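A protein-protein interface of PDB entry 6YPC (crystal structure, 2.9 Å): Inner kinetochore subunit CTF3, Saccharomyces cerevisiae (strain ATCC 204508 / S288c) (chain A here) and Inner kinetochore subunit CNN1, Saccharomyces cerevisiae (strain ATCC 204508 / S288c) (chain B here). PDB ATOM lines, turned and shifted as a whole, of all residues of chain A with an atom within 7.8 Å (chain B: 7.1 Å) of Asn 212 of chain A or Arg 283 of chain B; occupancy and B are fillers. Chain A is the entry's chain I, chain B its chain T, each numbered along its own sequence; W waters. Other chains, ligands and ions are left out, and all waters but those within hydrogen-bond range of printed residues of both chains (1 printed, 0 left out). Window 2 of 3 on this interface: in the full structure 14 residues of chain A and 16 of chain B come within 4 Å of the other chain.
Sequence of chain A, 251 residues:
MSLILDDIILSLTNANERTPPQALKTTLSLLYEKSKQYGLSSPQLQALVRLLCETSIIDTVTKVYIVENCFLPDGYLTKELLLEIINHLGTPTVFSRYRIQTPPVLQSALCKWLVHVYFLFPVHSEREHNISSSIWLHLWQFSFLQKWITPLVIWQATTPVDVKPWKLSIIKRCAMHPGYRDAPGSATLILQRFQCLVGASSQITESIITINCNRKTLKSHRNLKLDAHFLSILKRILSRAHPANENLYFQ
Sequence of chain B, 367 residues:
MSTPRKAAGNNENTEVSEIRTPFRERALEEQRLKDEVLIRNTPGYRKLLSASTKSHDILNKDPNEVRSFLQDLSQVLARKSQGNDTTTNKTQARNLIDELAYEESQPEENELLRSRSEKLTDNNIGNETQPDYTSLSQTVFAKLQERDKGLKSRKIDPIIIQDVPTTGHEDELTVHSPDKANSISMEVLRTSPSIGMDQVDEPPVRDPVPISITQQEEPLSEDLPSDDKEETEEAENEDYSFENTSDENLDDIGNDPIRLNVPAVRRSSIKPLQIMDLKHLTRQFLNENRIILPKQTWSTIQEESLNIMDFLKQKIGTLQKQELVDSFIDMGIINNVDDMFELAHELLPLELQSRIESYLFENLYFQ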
ATOM      1  N   MET A 176      11.889  -9.425 -11.449  1.00  0.00           N
ATOM      2  CA  MET A 176      11.379  -9.973 -12.701  1.00  0.00           C
ATOM      3  C   MET A 176      10.809 -11.372 -12.550  1.00  0.00           C
ATOM      4  O   MET A 176      10.191 -11.880 -13.494  1.00  0.00           O
ATOM      5  CB  MET A 176      12.504 -10.034 -13.731  1.00  0.00           C
ATOM      6  CG  MET A 176      13.245  -8.742 -13.948  1.00  0.00           C
ATOM      7  SD  MET A 176      12.153  -7.407 -14.456  1.00  0.00           S
ATOM      8  CE  MET A 176      11.478  -8.014 -16.006  1.00  0.00           C
ATOM      9  N   HIS A 177      11.031 -12.009 -11.418  1.00  0.00           N
ATOM     10  CA  HIS A 177      10.790 -13.438 -11.282  1.00  0.00           C
ATOM     11  C   HIS A 177       9.307 -13.712 -11.112  1.00  0.00           C
ATOM     12  O   HIS A 177       8.725 -13.285 -10.106  1.00  0.00           O
ATOM     13  CB  HIS A 177      11.566 -13.944 -10.080  1.00  0.00           C
ATOM     14  CG  HIS A 177      11.669 -15.425 -10.000  1.00  0.00           C
ATOM     15  ND1 HIS A 177      10.654 -16.263 -10.395  1.00  0.00           N
ATOM     16  CD2 HIS A 177      12.666 -16.221  -9.549  1.00  0.00           C
ATOM     17  CE1 HIS A 177      11.021 -17.517 -10.197  1.00  0.00           C
ATOM     18  NE2 HIS A 177      12.240 -17.519  -9.689  1.00  0.00           N
ATOM     19  N   PRO A 178       8.663 -14.422 -12.040  1.00  0.00           N
ATOM     20  CA  PRO A 178       7.270 -14.826 -11.819  1.00  0.00           C
ATOM     21  C   PRO A 178       7.200 -15.733 -10.605  1.00  0.00           C
ATOM     22  O   PRO A 178       8.211 -16.263 -10.133  1.00  0.00           O
ATOM     23  CB  PRO A 178       6.905 -15.579 -13.100  1.00  0.00           C
ATOM     24  CG  PRO A 178       8.206 -16.162 -13.557  1.00  0.00           C
ATOM     25  CD  PRO A 178       9.277 -15.157 -13.161  1.00  0.00           C
ATOM     26  N   PRO A 184       8.783  -6.739  -7.480  1.00  0.00           N
ATOM     27  CA  PRO A 184       9.134  -5.500  -8.197  1.00  0.00           C
ATOM     28  C   PRO A 184       9.012  -4.230  -7.351  1.00  0.00           C
ATOM     29  O   PRO A 184       9.875  -3.339  -7.446  1.00  0.00           O
ATOM     30  CB  PRO A 184       8.156  -5.498  -9.384  1.00  0.00           C
ATOM     31  CG  PRO A 184       7.191  -6.603  -9.117  1.00  0.00           C
ATOM     32  CD  PRO A 184       7.925  -7.593  -8.311  1.00  0.00           C
ATOM     33  N   GLY A 185       7.981  -4.120  -6.515  1.00  0.00           N
ATOM     34  CA  GLY A 185       7.867  -2.931  -5.700  1.00  0.00           C
ATOM     35  C   GLY A 185       9.020  -2.847  -4.721  1.00  0.00           C
ATOM     36  O   GLY A 185       9.800  -1.884  -4.718  1.00  0.00           O
ATOM     37  N   THR A 188      12.543  -2.215  -6.622  1.00  0.00           N
ATOM     38  CA  THR A 188      12.814  -0.832  -7.015  1.00  0.00           C
ATOM     39  C   THR A 188      13.186  -0.001  -5.803  1.00  0.00           C
ATOM     40  O   THR A 188      14.174   0.744  -5.833  1.00  0.00           O
ATOM     41  CB  THR A 188      11.615  -0.204  -7.727  1.00  0.00           C
ATOM     42  OG1 THR A 188      10.408  -0.661  -7.117  1.00  0.00           O
ATOM     43  CG2 THR A 188      11.607  -0.567  -9.187  1.00  0.00           C
ATOM     44  N   SER A 207      18.344  -0.994 -14.561  1.00  0.00           N
ATOM     45  CA  SER A 207      17.547  -2.041 -13.930  1.00  0.00           C
ATOM     46  C   SER A 207      16.182  -1.511 -13.551  1.00  0.00           C
ATOM     47  O   SER A 207      15.160  -2.159 -13.810  1.00  0.00           O
ATOM     48  CB  SER A 207      18.238  -2.589 -12.689  1.00  0.00           C
ATOM     49  OG  SER A 207      19.547  -3.009 -12.988  1.00  0.00           O
ATOM     50  N   ILE A 208      16.146  -0.319 -12.949  1.00  0.00           N
ATOM     51  CA  ILE A 208      14.870   0.222 -12.502  1.00  0.00           C
ATOM     52  C   ILE A 208      13.922   0.352 -13.679  1.00  0.00           C
ATOM     53  O   ILE A 208      12.717   0.115 -13.549  1.00  0.00           O
ATOM     54  CB  ILE A 208      15.065   1.564 -11.764  1.00  0.00           C
ATOM     55  CG1 ILE A 208      16.172   1.428 -10.721  1.00  0.00           C
ATOM     56  CG2 ILE A 208      13.802   1.931 -11.050  1.00  0.00           C
ATOM     57  CD1 ILE A 208      16.238   2.529  -9.733  1.00  0.00           C
ATOM     58  N   ILE A 209      14.452   0.675 -14.855  1.00  0.00           N
ATOM     59  CA  ILE A 209      13.606   0.799 -16.032  1.00  0.00           C
ATOM     60  C   ILE A 209      13.018  -0.553 -16.416  1.00  0.00           C
ATOM     61  O   ILE A 209      11.806  -0.682 -16.616  1.00  0.00           O
ATOM     62  CB  ILE A 209      14.409   1.422 -17.183  1.00  0.00           C
ATOM     63  CG1 ILE A 209      14.794   2.847 -16.816  1.00  0.00           C
ATOM     64  CG2 ILE A 209      13.605   1.406 -18.454  1.00  0.00           C
ATOM     65  CD1 ILE A 209      16.222   3.143 -17.020  1.00  0.00           C
ATOM     66  N   THR A 210      13.875  -1.582 -16.512  1.00  0.00           N
ATOM     67  CA  THR A 210      13.458  -2.945 -16.843  1.00  0.00           C
ATOM     68  C   THR A 210      12.332  -3.464 -15.952  1.00  0.00           C
ATOM     69  O   THR A 210      11.584  -4.357 -16.363  1.00  0.00           O
ATOM     70  CB  THR A 210      14.663  -3.885 -16.739  1.00  0.00           C
ATOM     71  OG1 THR A 210      15.836  -3.206 -17.210  1.00  0.00           O
ATOM     72  CG2 THR A 210      14.437  -5.143 -17.556  1.00  0.00           C
ATOM     73  N   ILE A 211      12.206  -2.942 -14.744  1.00  0.00           N
ATOM     74  CA  ILE A 211      11.101  -3.247 -13.854  1.00  0.00           C
ATOM     75  C   ILE A 211      10.152  -2.055 -13.910  1.00  0.00           C
ATOM     76  O   ILE A 211      10.379  -1.033 -13.249  1.00  0.00           O
ATOM     77  CB  ILE A 211      11.595  -3.494 -12.427  1.00  0.00           C
ATOM     78  CG1 ILE A 211      12.981  -4.109 -12.485  1.00  0.00           C
ATOM     79  CG2 ILE A 211      10.612  -4.339 -11.634  1.00  0.00           C
ATOM     80  CD1 ILE A 211      13.631  -4.195 -11.163  1.00  0.00           C
ATOM     81  N   ASN A 212       9.081  -2.165 -14.683  1.00  0.00           N
ATOM     82  CA  ASN A 212       8.070  -1.115 -14.713  1.00  0.00           C
ATOM     83  C   ASN A 212       7.069  -1.400 -13.601  1.00  0.00           C
ATOM     84  O   ASN A 212       6.389  -2.434 -13.625  1.00  0.00           O
ATOM     85  CB  ASN A 212       7.374  -1.038 -16.073  1.00  0.00           C
ATOM     86  CG  ASN A 212       8.178  -0.251 -17.114  1.00  0.00           C
ATOM     87  OD1 ASN A 212       9.115   0.479 -16.772  1.00  0.00           O
ATOM     88  ND2 ASN A 212       7.814  -0.407 -18.391  1.00  0.00           N
ATOM     89  N   CYS A 213       7.006  -0.497 -12.616  1.00  0.00           N
ATOM     90  CA  CYS A 213       5.967  -0.475 -11.586  1.00  0.00           C
ATOM     91  C   CYS A 213       5.086   0.757 -11.765  1.00  0.00           C
ATOM     92  O   CYS A 213       5.594   1.885 -11.822  1.00  0.00           O
ATOM     93  CB  CYS A 213       6.536  -0.475 -10.156  1.00  0.00           C
ATOM     94  SG  CYS A 213       7.869  -1.609  -9.740  1.00  0.00           S
ATOM     95  N   ASN A 214       3.764   0.532 -11.796  1.00  0.00           N
ATOM     96  CA  ASN A 214       2.689   1.517 -11.950  1.00  0.00           C
ATOM     97  C   ASN A 214       2.831   2.881 -11.266  1.00  0.00           C
ATOM     98  O   ASN A 214       1.924   3.711 -11.402  1.00  0.00           O
ATOM     99  CB  ASN A 214       1.374   0.909 -11.446  1.00  0.00           C
ATOM    100  CG  ASN A 214       1.442   0.505  -9.997  1.00  0.00           C
ATOM    101  OD1 ASN A 214       2.246   1.027  -9.221  1.00  0.00           O
ATOM    102  ND2 ASN A 214       0.585  -0.432  -9.616  1.00  0.00           N
ATOM    103  N   ARG A 215       3.908   3.114 -10.501  1.00  0.00           N
ATOM    104  CA  ARG A 215       4.127   4.361  -9.755  1.00  0.00           C
ATOM    105  C   ARG A 215       3.125   4.528  -8.609  1.00  0.00           C
ATOM    106  O   ARG A 215       3.162   5.540  -7.898  1.00  0.00           O
ATOM    107  CB  ARG A 215       4.055   5.602 -10.675  1.00  0.00           C
ATOM    108  CG  ARG A 215       4.955   5.542 -11.932  1.00  0.00           C
ATOM    109  CD  ARG A 215       4.774   6.765 -12.859  1.00  0.00           C
ATOM    110  NE  ARG A 215       5.956   7.623 -12.846  1.00  0.00           N
ATOM    111  CZ  ARG A 215       6.458   8.255 -13.904  1.00  0.00           C
ATOM    112  NH1 ARG A 215       5.884   8.150 -15.100  1.00  0.00           N
ATOM    113  NH2 ARG A 215       7.545   9.001 -13.757  1.00  0.00           N
ATOM    114  N   THR A 217       1.787   1.207  -6.886  1.00  0.00           N
ATOM    115  CA  THR A 217       2.298   0.189  -5.966  1.00  0.00           C
ATOM    116  C   THR A 217       3.533   0.684  -5.246  1.00  0.00           C
ATOM    117  O   THR A 217       3.781   0.306  -4.090  1.00  0.00           O
ATOM    118  CB  THR A 217       2.653  -1.116  -6.683  1.00  0.00           C
ATOM    119  OG1 THR A 217       3.222  -0.847  -7.971  1.00  0.00           O
ATOM    120  CG2 THR A 217       1.446  -2.022  -6.805  1.00  0.00           C
ATOM    121  N   ASP B 277      -1.802 -10.217 -16.431  1.00  0.00           N
ATOM    122  CA  ASP B 277      -1.258 -11.386 -15.741  1.00  0.00           C
ATOM    123  C   ASP B 277      -0.293 -12.168 -16.626  1.00  0.00           C
ATOM    124  O   ASP B 277       0.737 -12.659 -16.145  1.00  0.00           O
ATOM    125  CB  ASP B 277      -2.395 -12.291 -15.287  1.00  0.00           C
ATOM    126  CG  ASP B 277      -3.197 -11.688 -14.165  1.00  0.00           C
ATOM    127  OD1 ASP B 277      -2.620 -10.873 -13.406  1.00  0.00           O
ATOM    128  OD2 ASP B 277      -4.397 -12.027 -14.040  1.00  0.00           O
ATOM    129  N   LEU B 278      -0.632 -12.328 -17.910  1.00  0.00           N
ATOM    130  CA  LEU B 278       0.311 -12.911 -18.858  1.00  0.00           C
ATOM    131  C   LEU B 278       1.551 -12.040 -18.982  1.00  0.00           C
ATOM    132  O   LEU B 278       2.686 -12.525 -18.892  1.00  0.00           O
ATOM    133  CB  LEU B 278      -0.343 -13.074 -20.232  1.00  0.00           C
ATOM    134  CG  LEU B 278      -1.634 -13.883 -20.369  1.00  0.00           C
ATOM    135  CD1 LEU B 278      -2.170 -13.750 -21.780  1.00  0.00           C
ATOM    136  CD2 LEU B 278      -1.445 -15.355 -19.990  1.00  0.00           C
ATOM    137  N   LYS B 279       1.349 -10.739 -19.180  1.00  0.00           N
ATOM    138  CA  LYS B 279       2.484  -9.862 -19.367  1.00  0.00           C
ATOM    139  C   LYS B 279       3.405  -9.864 -18.156  1.00  0.00           C
ATOM    140  O   LYS B 279       4.517  -9.341 -18.249  1.00  0.00           O
ATOM    141  CB  LYS B 279       1.988  -8.452 -19.713  1.00  0.00           C
ATOM    142  CG  LYS B 279       2.789  -7.768 -20.836  1.00  0.00           C
ATOM    143  CD  LYS B 279       2.070  -6.555 -21.423  1.00  0.00           C
ATOM    144  CE  LYS B 279       3.053  -5.647 -22.170  1.00  0.00           C
ATOM    145  NZ  LYS B 279       2.444  -4.355 -22.626  1.00  0.00           N
ATOM    146  N   HIS B 280       2.999 -10.483 -17.047  1.00  0.00           N
ATOM    147  CA  HIS B 280       3.856 -10.648 -15.877  1.00  0.00           C
ATOM    148  C   HIS B 280       4.459 -12.043 -15.778  1.00  0.00           C
ATOM    149  O   HIS B 280       5.650 -12.180 -15.491  1.00  0.00           O
ATOM    150  CB  HIS B 280       3.078 -10.339 -14.596  1.00  0.00           C
ATOM    151  CG  HIS B 280       3.833 -10.646 -13.337  1.00  0.00           C
ATOM    152  ND1 HIS B 280       3.293 -11.390 -12.307  1.00  0.00           N
ATOM    153  CD2 HIS B 280       5.080 -10.299 -12.935  1.00  0.00           C
ATOM    154  CE1 HIS B 280       4.179 -11.496 -11.332  1.00  0.00           C
ATOM    155  NE2 HIS B 280       5.272 -10.842 -11.686  1.00  0.00           N
ATOM    156  N   LEU B 281       3.660 -13.088 -16.003  1.00  0.00           N
ATOM    157  CA  LEU B 281       4.183 -14.448 -15.962  1.00  0.00           C
ATOM    158  C   LEU B 281       5.338 -14.654 -16.922  1.00  0.00           C
ATOM    159  O   LEU B 281       6.095 -15.622 -16.776  1.00  0.00           O
ATOM    160  CB  LEU B 281       3.079 -15.438 -16.286  1.00  0.00           C
ATOM    161  CG  LEU B 281       1.924 -15.483 -15.296  1.00  0.00           C
ATOM    162  CD1 LEU B 281       1.204 -16.805 -15.426  1.00  0.00           C
ATOM    163  CD2 LEU B 281       2.453 -15.333 -13.899  1.00  0.00           C
ATOM    164  N   THR B 282       5.513 -13.757 -17.883  1.00  0.00           N
ATOM    165  CA  THR B 282       6.450 -14.000 -18.954  1.00  0.00           C
ATOM    166  C   THR B 282       7.382 -12.838 -19.257  1.00  0.00           C
ATOM    167  O   THR B 282       8.258 -12.999 -20.112  1.00  0.00           O
ATOM    168  CB  THR B 282       5.682 -14.382 -20.232  1.00  0.00           C
ATOM    169  OG1 THR B 282       4.470 -13.618 -20.305  1.00  0.00           O
ATOM    170  CG2 THR B 282       5.339 -15.870 -20.251  1.00  0.00           C
ATOM    171  N   ARG B 283       7.237 -11.680 -18.596  1.00  0.00           N
ATOM    172  CA  ARG B 283       8.011 -10.523 -19.051  1.00  0.00           C
ATOM    173  C   ARG B 283       9.517 -10.759 -18.917  1.00  0.00           C
ATOM    174  O   ARG B 283      10.306 -10.225 -19.708  1.00  0.00           O
ATOM    175  CB  ARG B 283       7.589  -9.244 -18.320  1.00  0.00           C
ATOM    176  CG  ARG B 283       7.909  -7.966 -19.129  1.00  0.00           C
ATOM    177  CD  ARG B 283       6.689  -7.041 -19.356  1.00  0.00           C
ATOM    178  NE  ARG B 283       7.078  -5.676 -19.747  1.00  0.00           N
ATOM    179  CZ  ARG B 283       6.395  -4.573 -19.435  1.00  0.00           C
ATOM    180  NH1 ARG B 283       5.281  -4.667 -18.718  1.00  0.00           N
ATOM    181  NH2 ARG B 283       6.828  -3.373 -19.831  1.00  0.00           N
ATOM    182  N   GLN B 284       9.935 -11.587 -17.964  1.00  0.00           N
ATOM    183  CA  GLN B 284      11.348 -11.929 -17.893  1.00  0.00           C
ATOM    184  C   GLN B 284      11.750 -12.816 -19.056  1.00  0.00           C
ATOM    185  O   GLN B 284      12.797 -12.607 -19.675  1.00  0.00           O
ATOM    186  CB  GLN B 284      11.652 -12.611 -16.564  1.00  0.00           C
ATOM    187  CG  GLN B 284      13.078 -13.107 -16.438  1.00  0.00           C
ATOM    188  CD  GLN B 284      14.126 -12.054 -16.786  1.00  0.00           C
ATOM    189  OE1 GLN B 284      13.889 -10.844 -16.694  1.00  0.00           O
ATOM    190  NE2 GLN B 284      15.296 -12.522 -17.206  1.00  0.00           N
ATOM    191  N   PHE B 285      10.916 -13.801 -19.370  1.00  0.00           N
ATOM    192  CA  PHE B 285      11.189 -14.707 -20.480  1.00  0.00           C
ATOM    193  C   PHE B 285      11.344 -13.959 -21.802  1.00  0.00           C
ATOM    194  O   PHE B 285      12.221 -14.284 -22.607  1.00  0.00           O
ATOM    195  CB  PHE B 285      10.063 -15.731 -20.564  1.00  0.00           C
ATOM    196  CG  PHE B 285      10.230 -16.721 -21.659  1.00  0.00           C
ATOM    197  CD1 PHE B 285      11.286 -17.616 -21.644  1.00  0.00           C
ATOM    198  CD2 PHE B 285       9.333 -16.766 -22.712  1.00  0.00           C
ATOM    199  CE1 PHE B 285      11.450 -18.539 -22.662  1.00  0.00           C
ATOM    200  CE2 PHE B 285       9.496 -17.683 -23.738  1.00  0.00           C
ATOM    201  CZ  PHE B 285      10.554 -18.578 -23.703  1.00  0.00           C
ATOM    202  N   LEU B 286      10.491 -12.961 -22.050  1.00  0.00           N
ATOM    203  CA  LEU B 286      10.573 -12.197 -23.294  1.00  0.00           C
ATOM    204  C   LEU B 286      11.846 -11.369 -23.343  1.00  0.00           C
ATOM    205  O   LEU B 286      12.580 -11.405 -24.336  1.00  0.00           O
ATOM    206  CB  LEU B 286       9.353 -11.289 -23.444  1.00  0.00           C
ATOM    207  CG  LEU B 286       8.027 -11.993 -23.185  1.00  0.00           C
ATOM    208  CD1 LEU B 286       6.863 -11.030 -23.335  1.00  0.00           C
ATOM    209  CD2 LEU B 286       7.903 -13.167 -24.135  1.00  0.00           C
ATOM    210  N   ASN B 287      12.107 -10.601 -22.280  1.00  0.00           N
ATOM    211  CA  ASN B 287      13.320  -9.793 -22.220  1.00  0.00           C
ATOM    212  C   ASN B 287      14.558 -10.660 -22.381  1.00  0.00           C
ATOM    213  O   ASN B 287      15.511 -10.283 -23.075  1.00  0.00           O
ATOM    214  CB  ASN B 287      13.376  -9.015 -20.902  1.00  0.00           C
ATOM    215  CG  ASN B 287      12.210  -8.066 -20.738  1.00  0.00           C
ATOM    216  OD1 ASN B 287      11.586  -7.658 -21.721  1.00  0.00           O
ATOM    217  ND2 ASN B 287      11.910  -7.701 -19.491  1.00  0.00           N
ATOM    218  N   GLU B 288      14.542 -11.848 -21.782  1.00  0.00           N
ATOM    219  CA  GLU B 288      15.716 -12.704 -21.810  1.00  0.00           C
ATOM    220  C   GLU B 288      15.979 -13.258 -23.207  1.00  0.00           C
ATOM    221  O   GLU B 288      17.069 -13.785 -23.473  1.00  0.00           O
ATOM    222  CB  GLU B 288      15.534 -13.816 -20.785  1.00  0.00           C
ATOM    223  CG  GLU B 288      16.684 -14.771 -20.684  1.00  0.00           C
ATOM    224  CD  GLU B 288      16.424 -15.894 -19.711  1.00  0.00           C
ATOM    225  OE1 GLU B 288      15.593 -15.705 -18.787  1.00  0.00           O
ATOM    226  OE2 GLU B 288      17.047 -16.970 -19.887  1.00  0.00           O
ATOM    227  N   ASN B 289      15.016 -13.131 -24.112  1.00  0.00           N
ATOM    228  CA  ASN B 289      15.273 -13.474 -25.501  1.00  0.00           C
ATOM    229  C   ASN B 289      15.081 -12.243 -26.380  1.00  0.00           C
ATOM    230  O   ASN B 289      15.461 -11.125 -26.013  1.00  0.00           O
ATOM    231  CB  ASN B 289      14.376 -14.630 -25.931  1.00  0.00           C
ATOM    232  CG  ASN B 289      14.463 -15.814 -24.975  1.00  0.00           C
ATOM    233  OD1 ASN B 289      15.308 -16.693 -25.140  1.00  0.00           O
ATOM    234  ND2 ASN B 289      13.583 -15.846 -23.978  1.00  0.00           N
ATOM    235  N   TRP B 298      -0.615  -9.542 -28.046  1.00  0.00           N
ATOM    236  CA  TRP B 298      -0.934  -9.832 -26.651  1.00  0.00           C
ATOM    237  C   TRP B 298      -2.338 -10.383 -26.511  1.00  0.00           C
ATOM    238  O   TRP B 298      -2.566 -11.366 -25.793  1.00  0.00           O
ATOM    239  CB  TRP B 298      -0.746  -8.574 -25.807  1.00  0.00           C
ATOM    240  CG  TRP B 298       0.668  -8.502 -25.384  1.00  0.00           C
ATOM    241  CD1 TRP B 298       1.609  -7.581 -25.757  1.00  0.00           C
ATOM    242  CD2 TRP B 298       1.336  -9.450 -24.555  1.00  0.00           C
ATOM    243  NE1 TRP B 298       2.819  -7.890 -25.184  1.00  0.00           N
ATOM    244  CE2 TRP B 298       2.676  -9.037 -24.445  1.00  0.00           C
ATOM    245  CE3 TRP B 298       0.924 -10.606 -23.880  1.00  0.00           C
ATOM    246  CZ2 TRP B 298       3.604  -9.737 -23.685  1.00  0.00           C
ATOM    247  CZ3 TRP B 298       1.846 -11.300 -23.128  1.00  0.00           C
ATOM    248  CH2 TRP B 298       3.170 -10.863 -23.030  1.00  0.00           C
HETATM  249  O   HOH W   1       7.440 -10.918 -10.542  1.00  0.00           O
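Asn 212 of chain A touches just one residue of chain B: Arg 283 (3.4 Å).
Of chain A, only Asn 212 comes within 4 Å of Arg 283 of chain B.
Of the printed residues of chain A, Gln 284 of chain B touches Met 176 (3.4 Å).
Printed residues of chain B within 4 Å of Pro 178 of chain A: Leu 281 (3.8 Å).
Of the printed residues of chain A, Asn 287 of chain B touches Met 176 (3.5 Å).
The nearest residue of chain A that does not touch Arg 283 of chain B is Met 176 of chain A (4.5 Å).
Among the printed residues, merely in contact across the chains: Met 176 of chain A with Gln 284 of chain B, Met 176 of chain A with Asn 287 of chain B and Pro 178 of chain A with Leu 281 of chain B.
Of the 14 printed residues of chain B, 4 touch a printed residue of chain A.
Of the 16 printed residues of chain A, 3 touch a printed residue of chain B.
Hydrophobic or aromatic side chains of chain A within 4 Å of the printed part of chain B: Met 176 and Pro 178.
Among the printed residues, no Asp or Glu carboxylate lies within 4 Å of a Lys or Arg side-chain nitrogen of the other chain.
The side-chain amide oxygen of Asn 212 of chain A sits close to the backbone carbonyl oxygen of Ile 209 of chain A (2.9 Å).
O of Arg 283 of chain B lies within hydrogen-bond range of ND2 of Asn 287 of chain B, at 3.0 Å.
Water W1 bridges NE2 of His 280 of chain B (2.5 Å) and O of His 177 of chain A (2.7 Å).
The guanidinium group (NH2) of Arg 283 of chain B sits close to the side-chain amide nitrogen (ND2) of Asn 212 of chain A (3.4 Å).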
